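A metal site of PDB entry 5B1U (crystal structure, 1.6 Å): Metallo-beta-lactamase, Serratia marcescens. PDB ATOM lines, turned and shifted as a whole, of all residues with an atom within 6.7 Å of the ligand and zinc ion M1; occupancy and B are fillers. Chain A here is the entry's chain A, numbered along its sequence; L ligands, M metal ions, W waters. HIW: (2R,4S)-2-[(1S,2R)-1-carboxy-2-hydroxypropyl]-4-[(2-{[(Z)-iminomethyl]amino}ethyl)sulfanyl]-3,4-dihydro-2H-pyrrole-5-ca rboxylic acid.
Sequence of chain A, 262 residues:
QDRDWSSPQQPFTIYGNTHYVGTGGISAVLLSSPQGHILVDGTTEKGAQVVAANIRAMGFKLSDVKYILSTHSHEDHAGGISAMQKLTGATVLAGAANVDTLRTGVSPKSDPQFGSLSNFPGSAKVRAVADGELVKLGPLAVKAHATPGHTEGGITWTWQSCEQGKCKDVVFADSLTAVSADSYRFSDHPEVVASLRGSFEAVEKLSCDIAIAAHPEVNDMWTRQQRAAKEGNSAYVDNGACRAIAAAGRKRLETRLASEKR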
ATOM      1  N   TRP A   5     -19.557 -30.160  -1.012  1.00  0.00           N
ATOM      2  CA  TRP A   5     -20.639 -29.991  -0.066  1.00  0.00           C
ATOM      3  C   TRP A   5     -20.431 -30.792   1.217  1.00  0.00           C
ATOM      4  O   TRP A   5     -21.036 -30.487   2.242  1.00  0.00           O
ATOM      5  CB  TRP A   5     -21.973 -30.488  -0.620  1.00  0.00           C
ATOM      6  CG  TRP A   5     -22.597 -29.722  -1.690  1.00  0.00           C
ATOM      7  CD1 TRP A   5     -22.283 -28.488  -2.081  1.00  0.00           C
ATOM      8  CD2 TRP A   5     -23.753 -30.124  -2.475  1.00  0.00           C
ATOM      9  NE1 TRP A   5     -23.114 -28.092  -3.102  1.00  0.00           N
ATOM     10  CE2 TRP A   5     -24.016 -29.079  -3.358  1.00  0.00           C
ATOM     11  CE3 TRP A   5     -24.521 -31.290  -2.557  1.00  0.00           C
ATOM     12  CZ2 TRP A   5     -25.035 -29.138  -4.320  1.00  0.00           C
ATOM     13  CZ3 TRP A   5     -25.552 -31.349  -3.500  1.00  0.00           C
ATOM     14  CH2 TRP A   5     -25.831 -30.256  -4.314  1.00  0.00           C
ATOM     15  N   ILE A  26     -20.948 -26.012   2.442  1.00  0.00           N
ATOM     16  CA  ILE A  26     -22.330 -25.735   2.908  1.00  0.00           C
ATOM     17  C   ILE A  26     -22.270 -25.259   4.350  1.00  0.00           C
ATOM     18  O   ILE A  26     -21.616 -25.867   5.196  1.00  0.00           O
ATOM     19  CB  ILE A  26     -23.265 -26.960   2.843  1.00  0.00           C
ATOM     20  CG1 ILE A  26     -23.359 -27.524   1.422  1.00  0.00           C
ATOM     21  CG2 ILE A  26     -24.622 -26.641   3.409  1.00  0.00           C
ATOM     22  CD1 ILE A  26     -24.129 -26.643   0.440  1.00  0.00           C
ATOM     23  N   HIS A  72     -33.947 -24.740   4.321  1.00  0.00           N
ATOM     24  CA  HIS A  72     -34.859 -25.378   3.420  1.00  0.00           C
ATOM     25  C   HIS A  72     -34.466 -26.816   3.125  1.00  0.00           C
ATOM     26  O   HIS A  72     -33.340 -27.253   3.370  1.00  0.00           O
ATOM     27  CB  HIS A  72     -35.047 -24.576   2.124  1.00  0.00           C
ATOM     28  CG  HIS A  72     -33.894 -24.659   1.175  1.00  0.00           C
ATOM     29  ND1 HIS A  72     -32.850 -23.758   1.193  1.00  0.00           N
ATOM     30  CD2 HIS A  72     -33.600 -25.541   0.189  1.00  0.00           C
ATOM     31  CE1 HIS A  72     -31.986 -24.071   0.251  1.00  0.00           C
ATOM     32  NE2 HIS A  72     -32.394 -25.163  -0.343  1.00  0.00           N
ATOM     33  N   HIS A  74     -33.621 -29.280   0.859  1.00  0.00           N
ATOM     34  CA  HIS A  74     -32.886 -29.970  -0.213  1.00  0.00           C
ATOM     35  C   HIS A  74     -31.706 -30.737   0.356  1.00  0.00           C
ATOM     36  O   HIS A  74     -31.208 -30.420   1.450  1.00  0.00           O
ATOM     37  CB  HIS A  74     -32.394 -28.980  -1.254  1.00  0.00           C
ATOM     38  CG  HIS A  74     -33.471 -28.396  -2.087  1.00  0.00           C
ATOM     39  ND1 HIS A  74     -33.346 -27.174  -2.686  1.00  0.00           N
ATOM     40  CD2 HIS A  74     -34.731 -28.827  -2.361  1.00  0.00           C
ATOM     41  CE1 HIS A  74     -34.445 -26.901  -3.365  1.00  0.00           C
ATOM     42  NE2 HIS A  74     -35.300 -27.900  -3.183  1.00  0.00           N
ATOM     43  N   GLU A  75     -31.222 -31.724  -0.409  1.00  0.00           N
ATOM     44  CA  GLU A  75     -30.178 -32.616   0.105  1.00  0.00           C
ATOM     45  C   GLU A  75     -28.944 -31.878   0.603  1.00  0.00           C
ATOM     46  O   GLU A  75     -28.249 -32.377   1.507  1.00  0.00           O
ATOM     47  CB  GLU A  75     -29.773 -33.661  -0.937  1.00  0.00           C
ATOM     48  CG  GLU A  75     -29.060 -33.060  -2.167  1.00  0.00           C
ATOM     49  CD  GLU A  75     -28.558 -34.069  -3.202  1.00  0.00           C
ATOM     50  OE1 GLU A  75     -28.043 -35.144  -2.822  1.00  0.00           O
ATOM     51  OE2 GLU A  75     -28.590 -33.734  -4.412  1.00  0.00           O
ATOM     52  N   ASP A  76     -28.600 -30.757  -0.013  1.00  0.00           N
ATOM     53  CA  ASP A  76     -27.335 -30.133   0.297  1.00  0.00           C
ATOM     54  C   ASP A  76     -27.338 -29.405   1.657  1.00  0.00           C
ATOM     55  O   ASP A  76     -26.288 -29.271   2.284  1.00  0.00           O
ATOM     56  CB  ASP A  76     -26.836 -29.246  -0.861  1.00  0.00           C
ATOM     57  CG  ASP A  76     -27.831 -28.235  -1.371  1.00  0.00           C
ATOM     58  OD1 ASP A  76     -29.048 -28.458  -1.353  1.00  0.00           O
ATOM     59  OD2 ASP A  76     -27.351 -27.196  -1.859  1.00  0.00           O
ATOM     60  N   HIS A  77     -28.535 -28.976   2.092  1.00  0.00           N
ATOM     61  CA  HIS A  77     -28.670 -28.238   3.374  1.00  0.00           C
ATOM     62  C   HIS A  77     -29.258 -29.095   4.475  1.00  0.00           C
ATOM     63  O   HIS A  77     -28.956 -28.911   5.667  1.00  0.00           O
ATOM     64  CB  HIS A  77     -29.551 -27.009   3.174  1.00  0.00           C
ATOM     65  CG  HIS A  77     -29.055 -26.122   2.078  1.00  0.00           C
ATOM     66  ND1 HIS A  77     -27.907 -25.351   2.192  1.00  0.00           N
ATOM     67  CD2 HIS A  77     -29.414 -26.069   0.761  1.00  0.00           C
ATOM     68  CE1 HIS A  77     -27.665 -24.785   1.018  1.00  0.00           C
ATOM     69  NE2 HIS A  77     -28.517 -25.257   0.129  1.00  0.00           N
ATOM     70  N   GLN A 113     -37.409 -27.355  -8.892  1.00  0.00           N
ATOM     71  CA  GLN A 113     -36.434 -28.369  -9.294  1.00  0.00           C
ATOM     72  C   GLN A 113     -36.983 -29.782  -9.296  1.00  0.00           C
ATOM     73  O   GLN A 113     -36.241 -30.702  -9.581  1.00  0.00           O
ATOM     74  CB  GLN A 113     -35.188 -28.264  -8.400  1.00  0.00           C
ATOM     75  CG  GLN A 113     -34.470 -26.938  -8.508  1.00  0.00           C
ATOM     76  CD  GLN A 113     -33.168 -26.939  -7.733  1.00  0.00           C
ATOM     77  OE1 GLN A 113     -32.164 -27.492  -8.189  1.00  0.00           O
ATOM     78  NE2 GLN A 113     -33.193 -26.375  -6.540  1.00  0.00           N
ATOM     79  N   SER A 116     -35.479 -33.143 -10.852  1.00  0.00           N
ATOM     80  CA  SER A 116     -34.043 -33.062 -10.896  1.00  0.00           C
ATOM     81  C   SER A 116     -33.369 -33.143  -9.502  1.00  0.00           C
ATOM     82  O   SER A 116     -32.141 -33.154  -9.418  1.00  0.00           O
ATOM     83  CB  SER A 116     -33.606 -31.796 -11.659  1.00  0.00           C
ATOM     84  OG  SER A 116     -33.783 -30.633 -10.857  1.00  0.00           O
ATOM     85  N   LEU A 117     -34.147 -33.303  -8.438  1.00  0.00           N
ATOM     86  CA  LEU A 117     -33.592 -33.309  -7.103  1.00  0.00           C
ATOM     87  C   LEU A 117     -33.286 -34.711  -6.665  1.00  0.00           C
ATOM     88  O   LEU A 117     -33.964 -35.656  -7.081  1.00  0.00           O
ATOM     89  CB  LEU A 117     -34.563 -32.714  -6.086  1.00  0.00           C
ATOM     90  CG  LEU A 117     -34.832 -31.233  -6.321  1.00  0.00           C
ATOM     91  CD1 LEU A 117     -36.144 -30.815  -5.662  1.00  0.00           C
ATOM     92  CD2 LEU A 117     -33.673 -30.415  -5.781  1.00  0.00           C
ATOM     93  N   SER A 118     -32.291 -34.865  -5.798  1.00  0.00           N
ATOM     94  CA  SER A 118     -32.020 -36.151  -5.186  1.00  0.00           C
ATOM     95  C   SER A 118     -32.666 -36.200  -3.811  1.00  0.00           C
ATOM     96  O   SER A 118     -32.590 -35.221  -3.041  1.00  0.00           O
ATOM     97  CB  SER A 118     -30.512 -36.345  -5.042  1.00  0.00           C
ATOM     98  OG  SER A 118     -29.905 -36.370  -6.315  1.00  0.00           O
ATOM     99  N   HIS A 150     -37.363 -20.373  -3.382  1.00  0.00           N
ATOM    100  CA  HIS A 150     -36.525 -21.515  -3.702  1.00  0.00           C
ATOM    101  C   HIS A 150     -37.231 -22.808  -3.226  1.00  0.00           C
ATOM    102  O   HIS A 150     -37.121 -23.845  -3.879  1.00  0.00           O
ATOM    103  CB  HIS A 150     -35.122 -21.300  -3.105  1.00  0.00           C
ATOM    104  CG  HIS A 150     -34.150 -22.391  -3.388  1.00  0.00           C
ATOM    105  ND1 HIS A 150     -33.363 -22.438  -4.525  1.00  0.00           N
ATOM    106  CD2 HIS A 150     -33.671 -23.364  -2.564  1.00  0.00           C
ATOM    107  CE1 HIS A 150     -32.522 -23.453  -4.430  1.00  0.00           C
ATOM    108  NE2 HIS A 150     -32.759 -24.075  -3.286  1.00  0.00           N
ATOM    109  N   ASP A 174     -31.305 -18.037   4.122  1.00  0.00           N
ATOM    110  CA  ASP A 174     -31.741 -19.093   3.203  1.00  0.00           C
ATOM    111  C   ASP A 174     -31.451 -18.717   1.758  1.00  0.00           C
ATOM    112  O   ASP A 174     -31.238 -17.546   1.430  1.00  0.00           O
ATOM    113  CB  ASP A 174     -33.236 -19.347   3.385  1.00  0.00           C
ATOM    114  CG  ASP A 174     -33.717 -20.602   2.722  1.00  0.00           C
ATOM    115  OD1 ASP A 174     -32.894 -21.469   2.409  1.00  0.00           O
ATOM    116  OD2 ASP A 174     -34.931 -20.662   2.504  1.00  0.00           O
ATOM    117  N   SER A 175     -31.380 -19.725   0.912  1.00  0.00           N
ATOM    118  CA  SER A 175     -31.248 -19.523  -0.539  1.00  0.00           C
ATOM    119  C   SER A 175     -32.435 -18.792  -1.108  1.00  0.00           C
ATOM    120  O   SER A 175     -33.574 -19.147  -0.856  1.00  0.00           O
ATOM    121  CB  SER A 175     -31.162 -20.856  -1.245  1.00  0.00           C
ATOM    122  OG  SER A 175     -31.250 -20.636  -2.639  1.00  0.00           O
ATOM    123  N   LEU A 176     -32.146 -17.832  -1.970  1.00  0.00           N
ATOM    124  CA  LEU A 176     -33.160 -17.054  -2.672  1.00  0.00           C
ATOM    125  C   LEU A 176     -33.108 -17.249  -4.175  1.00  0.00           C
ATOM    126  O   LEU A 176     -33.472 -16.343  -4.937  1.00  0.00           O
ATOM    127  CB  LEU A 176     -32.949 -15.583  -2.376  1.00  0.00           C
ATOM    128  CG  LEU A 176     -32.894 -15.188  -0.907  1.00  0.00           C
ATOM    129  CD1 LEU A 176     -32.621 -13.726  -0.708  1.00  0.00           C
ATOM    130  CD2 LEU A 176     -34.151 -15.643  -0.179  1.00  0.00           C
ATOM    131  N   THR A 177     -32.589 -18.406  -4.612  1.00  0.00           N
ATOM    132  CA  THR A 177     -32.242 -18.613  -6.012  1.00  0.00           C
ATOM    133  C   THR A 177     -33.363 -19.288  -6.818  1.00  0.00           C
ATOM    134  O   THR A 177     -33.898 -20.328  -6.451  1.00  0.00           O
ATOM    135  CB  THR A 177     -30.991 -19.481  -6.133  1.00  0.00           C
ATOM    136  OG1 THR A 177     -31.192 -20.708  -5.412  1.00  0.00           O
ATOM    137  CG2 THR A 177     -29.846 -18.750  -5.587  1.00  0.00           C
ATOM    138  N   VAL A 179     -33.852 -21.525  -9.510  1.00  0.00           N
ATOM    139  CA  VAL A 179     -33.232 -22.618 -10.274  1.00  0.00           C
ATOM    140  C   VAL A 179     -34.323 -23.672 -10.517  1.00  0.00           C
ATOM    141  O   VAL A 179     -35.232 -23.830  -9.701  1.00  0.00           O
ATOM    142  CB  VAL A 179     -32.020 -23.189  -9.488  1.00  0.00           C
ATOM    143  CG1 VAL A 179     -32.361 -23.469  -8.080  1.00  0.00           C
ATOM    144  CG2 VAL A 179     -31.449 -24.453 -10.110  1.00  0.00           C
ATOM    145  N   ALA A 214     -26.502 -19.782   3.287  1.00  0.00           N
ATOM    146  CA  ALA A 214     -26.573 -21.253   3.243  1.00  0.00           C
ATOM    147  C   ALA A 214     -25.474 -21.878   2.391  1.00  0.00           C
ATOM    148  O   ALA A 214     -24.809 -22.843   2.788  1.00  0.00           O
ATOM    149  CB  ALA A 214     -27.963 -21.693   2.818  1.00  0.00           C
ATOM    150  N   HIS A 215     -25.247 -21.282   1.213  1.00  0.00           N
ATOM    151  CA  HIS A 215     -24.019 -21.502   0.445  1.00  0.00           C
ATOM    152  C   HIS A 215     -23.038 -20.403   0.793  1.00  0.00           C
ATOM    153  O   HIS A 215     -23.265 -19.224   0.499  1.00  0.00           O
ATOM    154  CB  HIS A 215     -24.310 -21.483  -1.083  1.00  0.00           C
ATOM    155  CG  HIS A 215     -25.057 -22.667  -1.570  1.00  0.00           C
ATOM    156  ND1 HIS A 215     -24.435 -23.845  -1.899  1.00  0.00           N
ATOM    157  CD2 HIS A 215     -26.381 -22.939  -1.598  1.00  0.00           C
ATOM    158  CE1 HIS A 215     -25.330 -24.768  -2.166  1.00  0.00           C
ATOM    159  NE2 HIS A 215     -26.533 -24.245  -1.973  1.00  0.00           N
ATOM    160  N   GLU A 217     -20.201 -19.123   0.125  1.00  0.00           N
ATOM    161  CA  GLU A 217     -19.599 -18.210  -0.862  1.00  0.00           C
ATOM    162  C   GLU A 217     -20.526 -17.099  -1.355  1.00  0.00           C
ATOM    163  O   GLU A 217     -20.071 -16.072  -1.837  1.00  0.00           O
ATOM    164  CB  GLU A 217     -19.026 -18.986  -2.032  1.00  0.00           C
ATOM    165  CG  GLU A 217     -20.020 -19.482  -3.011  1.00  0.00           C
ATOM    166  CD  GLU A 217     -20.782 -20.738  -2.607  1.00  0.00           C
ATOM    167  OE1 GLU A 217     -20.545 -21.352  -1.533  1.00  0.00           O
ATOM    168  OE2 GLU A 217     -21.711 -21.034  -3.439  1.00  0.00           O
ATOM    169  N   VAL A 218     -21.824 -17.247  -1.097  1.00  0.00           N
ATOM    170  CA  VAL A 218     -22.774 -16.207  -1.478  1.00  0.00           C
ATOM    171  C   VAL A 218     -22.480 -14.886  -0.765  1.00  0.00           C
ATOM    172  O   VAL A 218     -22.607 -13.832  -1.392  1.00  0.00           O
ATOM    173  CB  VAL A 218     -24.217 -16.700  -1.239  1.00  0.00           C
ATOM    174  CG1 VAL A 218     -25.238 -15.573  -1.304  1.00  0.00           C
ATOM    175  CG2 VAL A 218     -24.541 -17.775  -2.235  1.00  0.00           C
ATOM    176  N   ALA A 248     -28.662 -10.171  -5.512  1.00  0.00           N
ATOM    177  CA  ALA A 248     -28.198 -11.266  -6.350  1.00  0.00           C
ATOM    178  C   ALA A 248     -29.368 -12.186  -6.674  1.00  0.00           C
ATOM    179  O   ALA A 248     -29.502 -12.634  -7.797  1.00  0.00           O
ATOM    180  CB  ALA A 248     -27.072 -11.989  -5.708  1.00  0.00           C
ATOM    181  N   ARG A 252     -30.859 -12.849 -10.487  1.00  0.00           N
ATOM    182  CA  ARG A 252     -30.968 -14.204 -11.031  1.00  0.00           C
ATOM    183  C   ARG A 252     -32.392 -14.435 -11.572  1.00  0.00           C
ATOM    184  O   ARG A 252     -32.592 -14.973 -12.642  1.00  0.00           O
ATOM    185  CB  ARG A 252     -30.619 -15.229  -9.950  1.00  0.00           C
ATOM    186  CG  ARG A 252     -30.655 -16.671 -10.453  1.00  0.00           C
ATOM    187  CD  ARG A 252     -30.009 -17.586  -9.417  1.00  0.00           C
ATOM    188  NE  ARG A 252     -29.904 -18.931  -9.942  1.00  0.00           N
ATOM    189  CZ  ARG A 252     -28.914 -19.774  -9.657  1.00  0.00           C
ATOM    190  NH1 ARG A 252     -28.025 -19.497  -8.718  1.00  0.00           N
ATOM    191  NH2 ARG A 252     -28.952 -20.983 -10.182  1.00  0.00           N
HETATM  192  O31 HIW L   1     -29.221 -21.763  -3.920  1.00  0.00           O
HETATM  193  C31 HIW L   1     -29.142 -22.965  -3.630  1.00  0.00           C
HETATM  194  O32 HIW L   1     -29.367 -23.352  -2.398  1.00  0.00           O
HETATM  195  C3  HIW L   1     -28.651 -23.893  -4.650  1.00  0.00           C
HETATM  196  N4  HIW L   1     -28.335 -25.086  -4.380  1.00  0.00           N
HETATM  197  C2  HIW L   1     -28.575 -23.534  -6.094  1.00  0.00           C
HETATM  198  C1  HIW L   1     -28.302 -24.906  -6.708  1.00  0.00           C
HETATM  199  C5  HIW L   1     -27.842 -25.826  -5.546  1.00  0.00           C
HETATM  200  C6  HIW L   1     -28.359 -27.260  -5.518  1.00  0.00           C
HETATM  201  C7  HIW L   1     -27.648 -28.065  -6.578  1.00  0.00           C
HETATM  202  O71 HIW L   1     -27.987 -29.207  -6.796  1.00  0.00           O
HETATM  203  O72 HIW L   1     -26.545 -27.629  -7.134  1.00  0.00           O
HETATM  204  C61 HIW L   1     -29.861 -27.393  -5.754  1.00  0.00           C
HETATM  205  O62 HIW L   1     -30.614 -26.334  -5.168  1.00  0.00           O
HETATM  206  C62 HIW L   1     -30.378 -28.712  -5.153  1.00  0.00           C
HETATM  207  S21 HIW L   1     -27.370 -22.212  -6.386  1.00  0.00           S
HETATM  208  C22 HIW L   1     -25.853 -22.748  -5.618  1.00  0.00           C
HETATM  209  C23 HIW L   1     -24.874 -21.614  -5.276  1.00  0.00           C
HETATM  210  N24 HIW L   1     -25.486 -20.393  -4.803  1.00  0.00           N
HETATM  211  C25 HIW L   1     -25.720 -19.356  -5.599  1.00  0.00           C
HETATM  212  N26 HIW L   1     -26.226 -18.324  -5.112  1.00  0.00           N
HETATM  213 ZN    ZN M   1     -28.373 -25.296  -2.034  1.00  0.00          ZN
HETATM  214 ZN    ZN M   2     -31.922 -25.692  -2.290  1.00  0.00          ZN
HETATM  215  O   HOH W   1     -26.051 -14.990  -4.595  1.00  0.00           O
HETATM  216  O   HOH W   2     -30.218 -31.407  -7.652  1.00  0.00           O
HETATM  217  O   HOH W   3     -30.147 -26.233  -2.439  1.00  0.00           O
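Water W3 lies within hydrogen-bond range of the side-chain carboxylate (OD1) of Asp 76 (2.7 Å) and an oxygen (O62) of the ligand (2.8 Å).
Water W2 bridges O of Ser 116 and O71 of the ligand.
Residues that only touch the ligand: Trp 5, His 72, His 74, Leu 117, His 150, Glu 217 and Val 218.
Hydrophobic or aromatic side chains that line the ligand: Trp 5, His 72, Leu 117, His 150, His 215 and Val 218.
14 residues have an atom within 4 Å of the ligand: Trp 5, His 72, His 74, Asp 76, His 77, Gln 113, Leu 117, His 150, Ser 175, Thr 177, His 215, Glu 217, Val 218 and Arg 252.
The nearest printed residue that does not touch the ligand is Val 179 (4.3 Å).
The side-chain hydroxyl of Ser 175 lies within hydrogen-bond range of the side-chain hydroxyl of Thr 177.
The side-chain hydroxyl (OG) of Ser 175 sits at hydrogen-bond distance from a ring nitrogen (ND1) of His 150 (3.4 Å).
O of Thr 177 sits at hydrogen-bond distance from ND1 of His 150, 2.9 Å away.
The backbone carbonyl oxygen (O) of Gln 113 sits at hydrogen-bond distance from the side-chain hydroxyl (OG) of Ser 116.
ND1 of His 72 sits at hydrogen-bond distance from OD1 of Asp 174, at 2.6 Å.
Three residues have an atom within 4 Å of zinc ion M1: Asp 76, His 77 and His 215.
Zinc ion M1 is bound by water W3 (2.0 Å), a ring nitrogen (NE2) of His 215 (2.1 Å), the side-chain carboxylate of Asp 76 (2.2 Å), a ring nitrogen (NE2) of His 77 (2.2 Å), an oxygen (O32) of the ligand (2.2 Å) and a nitrogen (N4) of the ligand (2.4 Å).
The side-chain hydroxyl of Ser 175 lies within hydrogen-bond range of an oxygen (O31) of the ligand (2.7 Å).
O31 of the ligand sits at hydrogen-bond distance from OG1 of Thr 177, at 2.7 Å.
The side-chain amide nitrogen of Gln 113 lies within hydrogen-bond range of an oxygen (O62) of the ligand.
The guanidinium group (NH1) of Arg 252 sits close to a sulfur (S21) of the ligand, at 3.6 Å.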
